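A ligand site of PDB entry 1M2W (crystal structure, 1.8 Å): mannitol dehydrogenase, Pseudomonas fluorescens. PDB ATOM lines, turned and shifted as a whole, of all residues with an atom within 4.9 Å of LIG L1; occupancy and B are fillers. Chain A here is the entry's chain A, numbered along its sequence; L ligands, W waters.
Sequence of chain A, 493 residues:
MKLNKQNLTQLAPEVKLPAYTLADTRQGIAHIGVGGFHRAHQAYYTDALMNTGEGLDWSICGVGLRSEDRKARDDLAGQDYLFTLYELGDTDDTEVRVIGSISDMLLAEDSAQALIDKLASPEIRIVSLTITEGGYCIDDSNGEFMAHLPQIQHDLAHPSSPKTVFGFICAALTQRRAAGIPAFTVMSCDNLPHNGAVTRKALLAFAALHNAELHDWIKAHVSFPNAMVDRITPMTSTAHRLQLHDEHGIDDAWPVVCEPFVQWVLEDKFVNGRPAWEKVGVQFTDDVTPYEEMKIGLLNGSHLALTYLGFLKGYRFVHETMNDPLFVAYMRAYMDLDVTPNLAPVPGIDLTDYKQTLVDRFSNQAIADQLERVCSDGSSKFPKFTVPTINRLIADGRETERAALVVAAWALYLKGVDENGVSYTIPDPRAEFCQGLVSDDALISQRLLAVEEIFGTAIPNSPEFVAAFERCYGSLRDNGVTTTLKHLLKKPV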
ATOM      1  N   PHE A  37      10.384 -18.523   4.696  1.00  0.00           N
ATOM      2  CA  PHE A  37       9.068 -17.987   5.019  1.00  0.00           C
ATOM      3  C   PHE A  37       8.625 -18.241   6.442  1.00  0.00           C
ATOM      4  O   PHE A  37       8.099 -17.348   7.114  1.00  0.00           O
ATOM      5  CB  PHE A  37       7.984 -18.497   4.072  1.00  0.00           C
ATOM      6  CG  PHE A  37       6.665 -17.827   4.292  1.00  0.00           C
ATOM      7  CD1 PHE A  37       6.553 -16.423   4.112  1.00  0.00           C
ATOM      8  CD2 PHE A  37       5.551 -18.548   4.705  1.00  0.00           C
ATOM      9  CE1 PHE A  37       5.310 -15.781   4.351  1.00  0.00           C
ATOM     10  CE2 PHE A  37       4.335 -17.928   4.950  1.00  0.00           C
ATOM     11  CZ  PHE A  37       4.202 -16.533   4.765  1.00  0.00           C
ATOM     12  N   GLU A 133       3.735 -25.406  -2.144  1.00  0.00           N
ATOM     13  CA  GLU A 133       2.445 -25.514  -2.798  1.00  0.00           C
ATOM     14  C   GLU A 133       2.088 -26.901  -3.319  1.00  0.00           C
ATOM     15  O   GLU A 133       0.910 -27.250  -3.382  1.00  0.00           O
ATOM     16  CB  GLU A 133       2.374 -24.516  -3.960  1.00  0.00           C
ATOM     17  CG  GLU A 133       2.414 -23.028  -3.454  1.00  0.00           C
ATOM     18  CD  GLU A 133       3.827 -22.505  -3.260  1.00  0.00           C
ATOM     19  OE1 GLU A 133       4.824 -23.258  -3.426  1.00  0.00           O
ATOM     20  OE2 GLU A 133       3.960 -21.312  -2.920  1.00  0.00           O
ATOM     21  N   ASN A 191       0.806 -21.404   0.543  1.00  0.00           N
ATOM     22  CA  ASN A 191      -0.119 -20.646  -0.313  1.00  0.00           C
ATOM     23  C   ASN A 191      -1.017 -21.469  -1.176  1.00  0.00           C
ATOM     24  O   ASN A 191      -0.704 -21.682  -2.347  1.00  0.00           O
ATOM     25  CB  ASN A 191       0.643 -19.773  -1.294  1.00  0.00           C
ATOM     26  CG  ASN A 191       1.441 -18.784  -0.628  1.00  0.00           C
ATOM     27  OD1 ASN A 191       0.896 -17.961   0.090  1.00  0.00           O
ATOM     28  ND2 ASN A 191       2.754 -18.811  -0.855  1.00  0.00           N
ATOM     29  N   VAL A 229      -1.511 -16.080   4.081  1.00  0.00           N
ATOM     30  CA  VAL A 229      -0.237 -15.697   4.661  1.00  0.00           C
ATOM     31  C   VAL A 229       0.528 -14.863   3.650  1.00  0.00           C
ATOM     32  O   VAL A 229       0.483 -15.153   2.473  1.00  0.00           O
ATOM     33  CB  VAL A 229       0.594 -16.962   5.006  1.00  0.00           C
ATOM     34  CG1 VAL A 229      -0.150 -17.751   6.126  1.00  0.00           C
ATOM     35  CG2 VAL A 229       0.753 -17.853   3.761  1.00  0.00           C
ATOM     36  N   ASP A 230       1.238 -13.829   4.099  1.00  0.00           N
ATOM     37  CA  ASP A 230       1.924 -12.959   3.130  1.00  0.00           C
ATOM     38  C   ASP A 230       3.182 -12.272   3.689  1.00  0.00           C
ATOM     39  O   ASP A 230       3.101 -11.573   4.704  1.00  0.00           O
ATOM     40  CB  ASP A 230       0.929 -11.845   2.672  1.00  0.00           C
ATOM     41  CG  ASP A 230       1.446 -10.983   1.498  1.00  0.00           C
ATOM     42  OD1 ASP A 230       2.524 -11.278   0.934  1.00  0.00           O
ATOM     43  OD2 ASP A 230       0.757  -9.992   1.133  1.00  0.00           O
ATOM     44  N   ARG A 231       4.337 -12.522   3.041  1.00  0.00           N
ATOM     45  CA  ARG A 231       5.560 -11.803   3.334  1.00  0.00           C
ATOM     46  C   ARG A 231       6.596 -12.239   2.285  1.00  0.00           C
ATOM     47  O   ARG A 231       6.934 -13.425   2.224  1.00  0.00           O
ATOM     48  CB  ARG A 231       6.126 -12.071   4.725  1.00  0.00           C
ATOM     49  CG  ARG A 231       7.261 -11.053   5.040  1.00  0.00           C
ATOM     50  CD  ARG A 231       7.669 -11.016   6.487  1.00  0.00           C
ATOM     51  NE  ARG A 231       8.069  -9.649   6.864  1.00  0.00           N
ATOM     52  CZ  ARG A 231       8.327  -9.251   8.103  1.00  0.00           C
ATOM     53  NH1 ARG A 231       8.275 -10.101   9.112  1.00  0.00           N
ATOM     54  NH2 ARG A 231       8.606  -7.968   8.347  1.00  0.00           N
ATOM     55  N   ILE A 232       7.060 -11.302   1.449  1.00  0.00           N
ATOM     56  CA  ILE A 232       8.044 -11.655   0.440  1.00  0.00           C
ATOM     57  C   ILE A 232       9.378 -11.934   1.132  1.00  0.00           C
ATOM     58  O   ILE A 232       9.889 -11.102   1.891  1.00  0.00           O
ATOM     59  CB  ILE A 232       8.152 -10.547  -0.605  1.00  0.00           C
ATOM     60  CG1 ILE A 232       6.805 -10.446  -1.364  1.00  0.00           C
ATOM     61  CG2 ILE A 232       9.329 -10.819  -1.567  1.00  0.00           C
ATOM     62  CD1 ILE A 232       6.708  -9.173  -2.220  1.00  0.00           C
ATOM     63  N   THR A 233       9.912 -13.112   0.861  1.00  0.00           N
ATOM     64  CA  THR A 233      11.157 -13.582   1.499  1.00  0.00           C
ATOM     65  C   THR A 233      12.054 -14.226   0.425  1.00  0.00           C
ATOM     66  O   THR A 233      11.815 -15.355  -0.003  1.00  0.00           O
ATOM     67  CB  THR A 233      10.784 -14.666   2.582  1.00  0.00           C
ATOM     68  OG1 THR A 233       9.798 -14.098   3.479  1.00  0.00           O
ATOM     69  CG2 THR A 233      12.017 -15.080   3.423  1.00  0.00           C
ATOM     70  N   LYS A 295      -5.308 -12.244  -2.274  1.00  0.00           N
ATOM     71  CA  LYS A 295      -3.843 -12.313  -2.248  1.00  0.00           C
ATOM     72  C   LYS A 295      -3.238 -13.325  -3.211  1.00  0.00           C
ATOM     73  O   LYS A 295      -2.268 -13.032  -3.930  1.00  0.00           O
ATOM     74  CB  LYS A 295      -3.357 -12.516  -0.794  1.00  0.00           C
ATOM     75  CG  LYS A 295      -1.820 -12.406  -0.605  1.00  0.00           C
ATOM     76  CD  LYS A 295      -1.243 -13.847  -0.610  1.00  0.00           C
ATOM     77  CE  LYS A 295       0.307 -13.841  -0.687  1.00  0.00           C
ATOM     78  NZ  LYS A 295       0.796 -15.310  -0.508  1.00  0.00           N
ATOM     79  N   LEU A 299      -1.487 -11.233  -5.968  1.00  0.00           N
ATOM     80  CA  LEU A 299      -0.026 -11.229  -5.726  1.00  0.00           C
ATOM     81  C   LEU A 299       0.660 -12.450  -6.342  1.00  0.00           C
ATOM     82  O   LEU A 299       1.541 -12.324  -7.238  1.00  0.00           O
ATOM     83  CB  LEU A 299       0.278 -11.164  -4.221  1.00  0.00           C
ATOM     84  CG  LEU A 299       1.738 -10.832  -3.833  1.00  0.00           C
ATOM     85  CD1 LEU A 299       1.772 -10.461  -2.319  1.00  0.00           C
ATOM     86  CD2 LEU A 299       2.656 -11.995  -4.145  1.00  0.00           C
ATOM     87  N   ASN A 300       0.288 -13.644  -5.907  1.00  0.00           N
ATOM     88  CA  ASN A 300       0.970 -14.828  -6.451  1.00  0.00           C
ATOM     89  C   ASN A 300       0.735 -14.968  -7.971  1.00  0.00           C
ATOM     90  O   ASN A 300       1.631 -15.391  -8.735  1.00  0.00           O
ATOM     91  CB  ASN A 300       0.514 -16.066  -5.647  1.00  0.00           C
ATOM     92  CG  ASN A 300       0.936 -16.011  -4.206  1.00  0.00           C
ATOM     93  OD1 ASN A 300       0.101 -15.909  -3.317  1.00  0.00           O
ATOM     94  ND2 ASN A 300       2.262 -16.104  -3.956  1.00  0.00           N
ATOM     95  N   HIS A 303       3.061 -12.522  -9.670  1.00  0.00           N
ATOM     96  CA  HIS A 303       4.418 -13.063  -9.654  1.00  0.00           C
ATOM     97  C   HIS A 303       4.622 -14.051 -10.827  1.00  0.00           C
ATOM     98  O   HIS A 303       5.650 -13.985 -11.544  1.00  0.00           O
ATOM     99  CB  HIS A 303       4.671 -13.813  -8.323  1.00  0.00           C
ATOM    100  CG  HIS A 303       5.522 -13.060  -7.337  1.00  0.00           C
ATOM    101  ND1 HIS A 303       5.660 -13.476  -6.031  1.00  0.00           N
ATOM    102  CD2 HIS A 303       6.237 -11.908  -7.452  1.00  0.00           C
ATOM    103  CE1 HIS A 303       6.448 -12.627  -5.380  1.00  0.00           C
ATOM    104  NE2 HIS A 303       6.802 -11.659  -6.222  1.00  0.00           N
ATOM    105  N   LEU A 304       3.702 -15.001 -11.059  1.00  0.00           N
ATOM    106  CA  LEU A 304       3.924 -15.921 -12.196  1.00  0.00           C
ATOM    107  C   LEU A 304       3.882 -15.181 -13.548  1.00  0.00           C
ATOM    108  O   LEU A 304       4.635 -15.514 -14.490  1.00  0.00           O
ATOM    109  CB  LEU A 304       2.894 -17.069 -12.229  1.00  0.00           C
ATOM    110  CG  LEU A 304       2.996 -18.080 -11.071  1.00  0.00           C
ATOM    111  CD1 LEU A 304       2.261 -19.384 -11.487  1.00  0.00           C
ATOM    112  CD2 LEU A 304       4.474 -18.431 -10.746  1.00  0.00           C
ATOM    113  N   ARG A 361       5.326  -2.981  -3.543  1.00  0.00           N
ATOM    114  CA  ARG A 361       6.095  -4.049  -2.902  1.00  0.00           C
ATOM    115  C   ARG A 361       6.978  -4.805  -3.877  1.00  0.00           C
ATOM    116  O   ARG A 361       8.123  -5.145  -3.540  1.00  0.00           O
ATOM    117  CB  ARG A 361       5.151  -5.008  -2.141  1.00  0.00           C
ATOM    118  CG  ARG A 361       4.516  -4.364  -0.911  1.00  0.00           C
ATOM    119  CD  ARG A 361       3.391  -5.211  -0.296  1.00  0.00           C
ATOM    120  NE  ARG A 361       3.862  -6.571  -0.039  1.00  0.00           N
ATOM    121  CZ  ARG A 361       3.052  -7.622   0.043  1.00  0.00           C
ATOM    122  NH1 ARG A 361       1.723  -7.472  -0.083  1.00  0.00           N
ATOM    123  NH2 ARG A 361       3.592  -8.806   0.257  1.00  0.00           N
ATOM    124  N   ARG A 373      13.696 -17.921  -7.791  1.00  0.00           N
ATOM    125  CA  ARG A 373      12.840 -18.356  -6.706  1.00  0.00           C
ATOM    126  C   ARG A 373      11.348 -18.363  -7.120  1.00  0.00           C
ATOM    127  O   ARG A 373      10.627 -19.356  -6.912  1.00  0.00           O
ATOM    128  CB  ARG A 373      12.995 -17.404  -5.487  1.00  0.00           C
ATOM    129  CG  ARG A 373      12.209 -17.861  -4.272  1.00  0.00           C
ATOM    130  CD  ARG A 373      12.240 -16.803  -3.185  1.00  0.00           C
ATOM    131  NE  ARG A 373      11.350 -15.653  -3.505  1.00  0.00           N
ATOM    132  CZ  ARG A 373      10.031 -15.674  -3.321  1.00  0.00           C
ATOM    133  NH1 ARG A 373       9.437 -16.779  -2.826  1.00  0.00           N
ATOM    134  NH2 ARG A 373       9.317 -14.574  -3.578  1.00  0.00           N
ATOM    135  N   VAL A 374      10.909 -17.258  -7.701  1.00  0.00           N
ATOM    136  CA  VAL A 374       9.503 -17.121  -8.113  1.00  0.00           C
ATOM    137  C   VAL A 374       9.204 -18.143  -9.234  1.00  0.00           C
ATOM    138  O   VAL A 374       8.144 -18.767  -9.219  1.00  0.00           O
ATOM    139  CB  VAL A 374       9.211 -15.683  -8.563  1.00  0.00           C
ATOM    140  CG1 VAL A 374       7.730 -15.541  -8.922  1.00  0.00           C
ATOM    141  CG2 VAL A 374       9.531 -14.743  -7.438  1.00  0.00           C
ATOM    142  N   LYS A 381       2.863 -24.590  -8.833  1.00  0.00           N
ATOM    143  CA  LYS A 381       2.270 -23.253  -8.636  1.00  0.00           C
ATOM    144  C   LYS A 381       1.146 -22.895  -9.606  1.00  0.00           C
ATOM    145  O   LYS A 381       0.177 -22.223  -9.208  1.00  0.00           O
ATOM    146  CB  LYS A 381       3.364 -22.188  -8.732  1.00  0.00           C
ATOM    147  CG  LYS A 381       4.331 -22.197  -7.519  1.00  0.00           C
ATOM    148  CD  LYS A 381       5.551 -21.280  -7.771  1.00  0.00           C
ATOM    149  CE  LYS A 381       6.484 -21.217  -6.515  1.00  0.00           C
ATOM    150  NZ  LYS A 381       7.732 -20.469  -6.915  1.00  0.00           N
ATOM    151  N   PHE A 385      -2.026 -20.702  -8.433  1.00  0.00           N
ATOM    152  CA  PHE A 385      -1.952 -19.255  -8.640  1.00  0.00           C
ATOM    153  C   PHE A 385      -2.606 -18.672  -9.874  1.00  0.00           C
ATOM    154  O   PHE A 385      -3.011 -17.508  -9.891  1.00  0.00           O
ATOM    155  CB  PHE A 385      -0.469 -18.820  -8.729  1.00  0.00           C
ATOM    156  CG  PHE A 385       0.381 -19.140  -7.506  1.00  0.00           C
ATOM    157  CD1 PHE A 385       1.750 -18.927  -7.563  1.00  0.00           C
ATOM    158  CD2 PHE A 385      -0.176 -19.598  -6.297  1.00  0.00           C
ATOM    159  CE1 PHE A 385       2.593 -19.162  -6.444  1.00  0.00           C
ATOM    160  CE2 PHE A 385       0.649 -19.843  -5.152  1.00  0.00           C
ATOM    161  CZ  PHE A 385       2.049 -19.611  -5.242  1.00  0.00           C
HETATM  162  O1  LIG L   1       3.644 -13.558   0.384  1.00  0.00           O
HETATM  163  C1  LIG L   1       4.234 -13.532  -0.934  1.00  0.00           C
HETATM  164  C2  LIG L   1       4.610 -14.963  -1.298  1.00  0.00           C
HETATM  165  O2  LIG L   1       3.443 -15.838  -1.290  1.00  0.00           O
HETATM  166  C3  LIG L   1       5.344 -15.010  -2.643  1.00  0.00           C
HETATM  167  O3  LIG L   1       6.651 -14.397  -2.443  1.00  0.00           O
HETATM  168  C4  LIG L   1       5.513 -16.479  -3.108  1.00  0.00           C
HETATM  169  O4  LIG L   1       6.549 -17.113  -2.358  1.00  0.00           O
HETATM  170  C5  LIG L   1       5.900 -16.509  -4.589  1.00  0.00           C
HETATM  171  O5  LIG L   1       4.820 -16.000  -5.382  1.00  0.00           O
HETATM  172  C6  LIG L   1       6.267 -17.966  -5.058  1.00  0.00           C
HETATM  173  O6  LIG L   1       6.364 -17.951  -6.475  1.00  0.00           O
HETATM  174  P1  LG2 L   2      12.682 -22.409   1.505  1.00  0.00           P
HETATM  175  O1  LG2 L   2      13.176 -22.990   0.283  1.00  0.00           O
HETATM  176  O2  LG2 L   2      13.460 -21.415   2.382  1.00  0.00           O
HETATM  177  O3  LG2 L   2      12.209 -23.601   2.482  1.00  0.00           O
HETATM  178  C1  LG2 L   2      11.237 -24.569   1.990  1.00  0.00           C
HETATM  179  C2  LG2 L   2      11.110 -25.510   3.227  1.00  0.00           C
HETATM  180  O4  LG2 L   2      10.108 -26.560   2.862  1.00  0.00           O
HETATM  181  C3  LG2 L   2      12.365 -26.353   3.536  1.00  0.00           C
HETATM  182  O5  LG2 L   2      12.271 -26.599   4.931  1.00  0.00           O
HETATM  183  C4  LG2 L   2      12.165 -27.593   2.684  1.00  0.00           C
HETATM  184  O6  LG2 L   2      13.012 -28.718   2.983  1.00  0.00           O
HETATM  185  C5  LG2 L   2      10.693 -27.865   2.972  1.00  0.00           C
HETATM  186  N1  LG2 L   2      10.077 -28.751   2.023  1.00  0.00           N
HETATM  187  C6  LG2 L   2      10.079 -28.778   0.634  1.00  0.00           C
HETATM  188  N2  LG2 L   2       9.360 -29.769   0.111  1.00  0.00           N
HETATM  189  C7  LG2 L   2       8.854 -30.410   1.248  1.00  0.00           C
HETATM  190  C8  LG2 L   2       8.014 -31.519   1.344  1.00  0.00           C
HETATM  191  N3  LG2 L   2       7.491 -32.191   0.315  1.00  0.00           N
HETATM  192  N4  LG2 L   2       7.673 -31.970   2.646  1.00  0.00           N
HETATM  193  C9  LG2 L   2       8.153 -31.328   3.797  1.00  0.00           C
HETATM  194  N5  LG2 L   2       8.994 -30.210   3.744  1.00  0.00           N
HETATM  195  C10 LG2 L   2       9.312 -29.797   2.435  1.00  0.00           C
HETATM  196  O7  LG2 L   2      11.299 -21.694   1.155  1.00  0.00           O
HETATM  197  P2  LG2 L   2      10.342 -20.642   1.878  1.00  0.00           P
HETATM  198  O8  LG2 L   2      10.678 -19.245   1.509  1.00  0.00           O
HETATM  199  O9  LG2 L   2      10.374 -20.981   3.314  1.00  0.00           O
HETATM  200  O10 LG2 L   2       8.917 -21.018   1.200  1.00  0.00           O
HETATM  201  C11 LG2 L   2       8.249 -22.208   1.748  1.00  0.00           C
HETATM  202  C12 LG2 L   2       6.753 -22.159   1.498  1.00  0.00           C
HETATM  203  O11 LG2 L   2       6.008 -21.251   2.354  1.00  0.00           O
HETATM  204  C13 LG2 L   2       6.258 -21.855   0.042  1.00  0.00           C
HETATM  205  O12 LG2 L   2       6.382 -22.965  -0.812  1.00  0.00           O
HETATM  206  C14 LG2 L   2       4.844 -21.285   0.229  1.00  0.00           C
HETATM  207  O13 LG2 L   2       3.730 -22.223   0.207  1.00  0.00           O
HETATM  208  C15 LG2 L   2       4.974 -20.544   1.543  1.00  0.00           C
HETATM  209  N6  LG2 L   2       5.349 -19.117   1.368  1.00  0.00           N
HETATM  210  C16 LG2 L   2       6.620 -18.572   0.961  1.00  0.00           C
HETATM  211  C17 LG2 L   2       6.683 -17.166   0.824  1.00  0.00           C
HETATM  212  C18 LG2 L   2       7.975 -16.500   0.340  1.00  0.00           C
HETATM  213  O14 LG2 L   2       7.960 -15.193   0.060  1.00  0.00           O
HETATM  214  N7  LG2 L   2       9.001 -17.285   0.171  1.00  0.00           N
HETATM  215  C19 LG2 L   2       5.518 -16.350   1.072  1.00  0.00           C
HETATM  216  C20 LG2 L   2       4.301 -16.961   1.482  1.00  0.00           C
HETATM  217  C21 LG2 L   2       4.201 -18.323   1.621  1.00  0.00           C
HETATM  218  O   HOH W   1       6.339 -19.810  -2.246  1.00  0.00           O
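An oxygen (O6) of LIG L1 sits at hydrogen-bond distance from the side-chain amino group (NZ) of Lys 381 (2.9 Å). The backbone NH of Thr 233 sits at hydrogen-bond distance from an oxygen (O14) of LG2 L2. An oxygen (O2) of LIG L1 lies within hydrogen-bond range of the side-chain amide nitrogen (ND2) of Asn 300 (2.9 Å). NZ of Lys 295 sits at hydrogen-bond distance from O2 of LIG L1, 2.8 Å away. O1 of LIG L1 is in hydrogen-bond range of OD1 of Asp 230, at 2.6 Å. The side-chain carboxylate of Glu 133 sits at hydrogen-bond distance from an oxygen (O12) of LG2 L2 (3.1 Å). The guanidinium group (NH2) of Arg 373 is in hydrogen-bond range of an oxygen (O3) of LIG L1 (2.9 Å). An oxygen (O5) of LIG L1 is in hydrogen-bond range of a ring nitrogen (ND1) of His 303 (2.7 Å). The side-chain amide nitrogen of Asn 191 is in hydrogen-bond range of an oxygen (O2) of LIG L1 (3.1 Å). The backbone NH (N) of Phe 37 is in hydrogen-bond range of an oxygen (O9) of LG2 L2 (2.8 Å). O of Thr 233 lies within hydrogen-bond range of N7 of LG2 L2, 3.4 Å away. The backbone NH of Arg 231 is in hydrogen-bond range of an oxygen (O1) of LIG L1, at 2.9 Å. O of Val 374 is in hydrogen-bond range of O6 of LIG L1 (3.4 Å). N of Asn 191 sits at hydrogen-bond distance from O13 of LG2 L2 (3.1 Å).
The side-chain amide nitrogen (ND2) of Asn 191 is in hydrogen-bond range of the side-chain carboxylate (OE2) of Glu 133. OG1 of Thr 233 sits at hydrogen-bond distance from O of Arg 231 (3.2 Å). The side-chain amino group of Lys 295 is in hydrogen-bond range of the backbone carbonyl oxygen of Val 229 (3.0 Å). NZ of Lys 295 sits at hydrogen-bond distance from OD1 of Asn 300 (3.0 Å). The side-chain amino group of Lys 381 lies within hydrogen-bond range of the backbone carbonyl oxygen of Arg 373 (3.1 Å). The side-chain amino group (NZ) of Lys 295 sits at hydrogen-bond distance from the side-chain amide oxygen (OD1) of Asn 191 (2.7 Å). The side-chain amino group (NZ) of Lys 381 lies within hydrogen-bond range of the backbone carbonyl oxygen (O) of Val 374, 2.9 Å away. The guanidinium group (NH2) of Arg 361 is in salt-bridge range of the side-chain carboxylate (OD1) of Asp 230 (2.8 Å).
Merely in contact with LIG L1: Leu 299 (3.9 Å) and Phe 385 (3.96 Å).
An oxygen (O14) of LG2 L2 lies within hydrogen-bond range of an oxygen (O3) of LIG L1 (2.9 Å).
Water W1 lies within hydrogen-bond range of O4 of LIG L1 (2.7 Å), OE2 of Glu 133 (2.9 Å) and O12 of LG2 L2 (3.5 Å).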
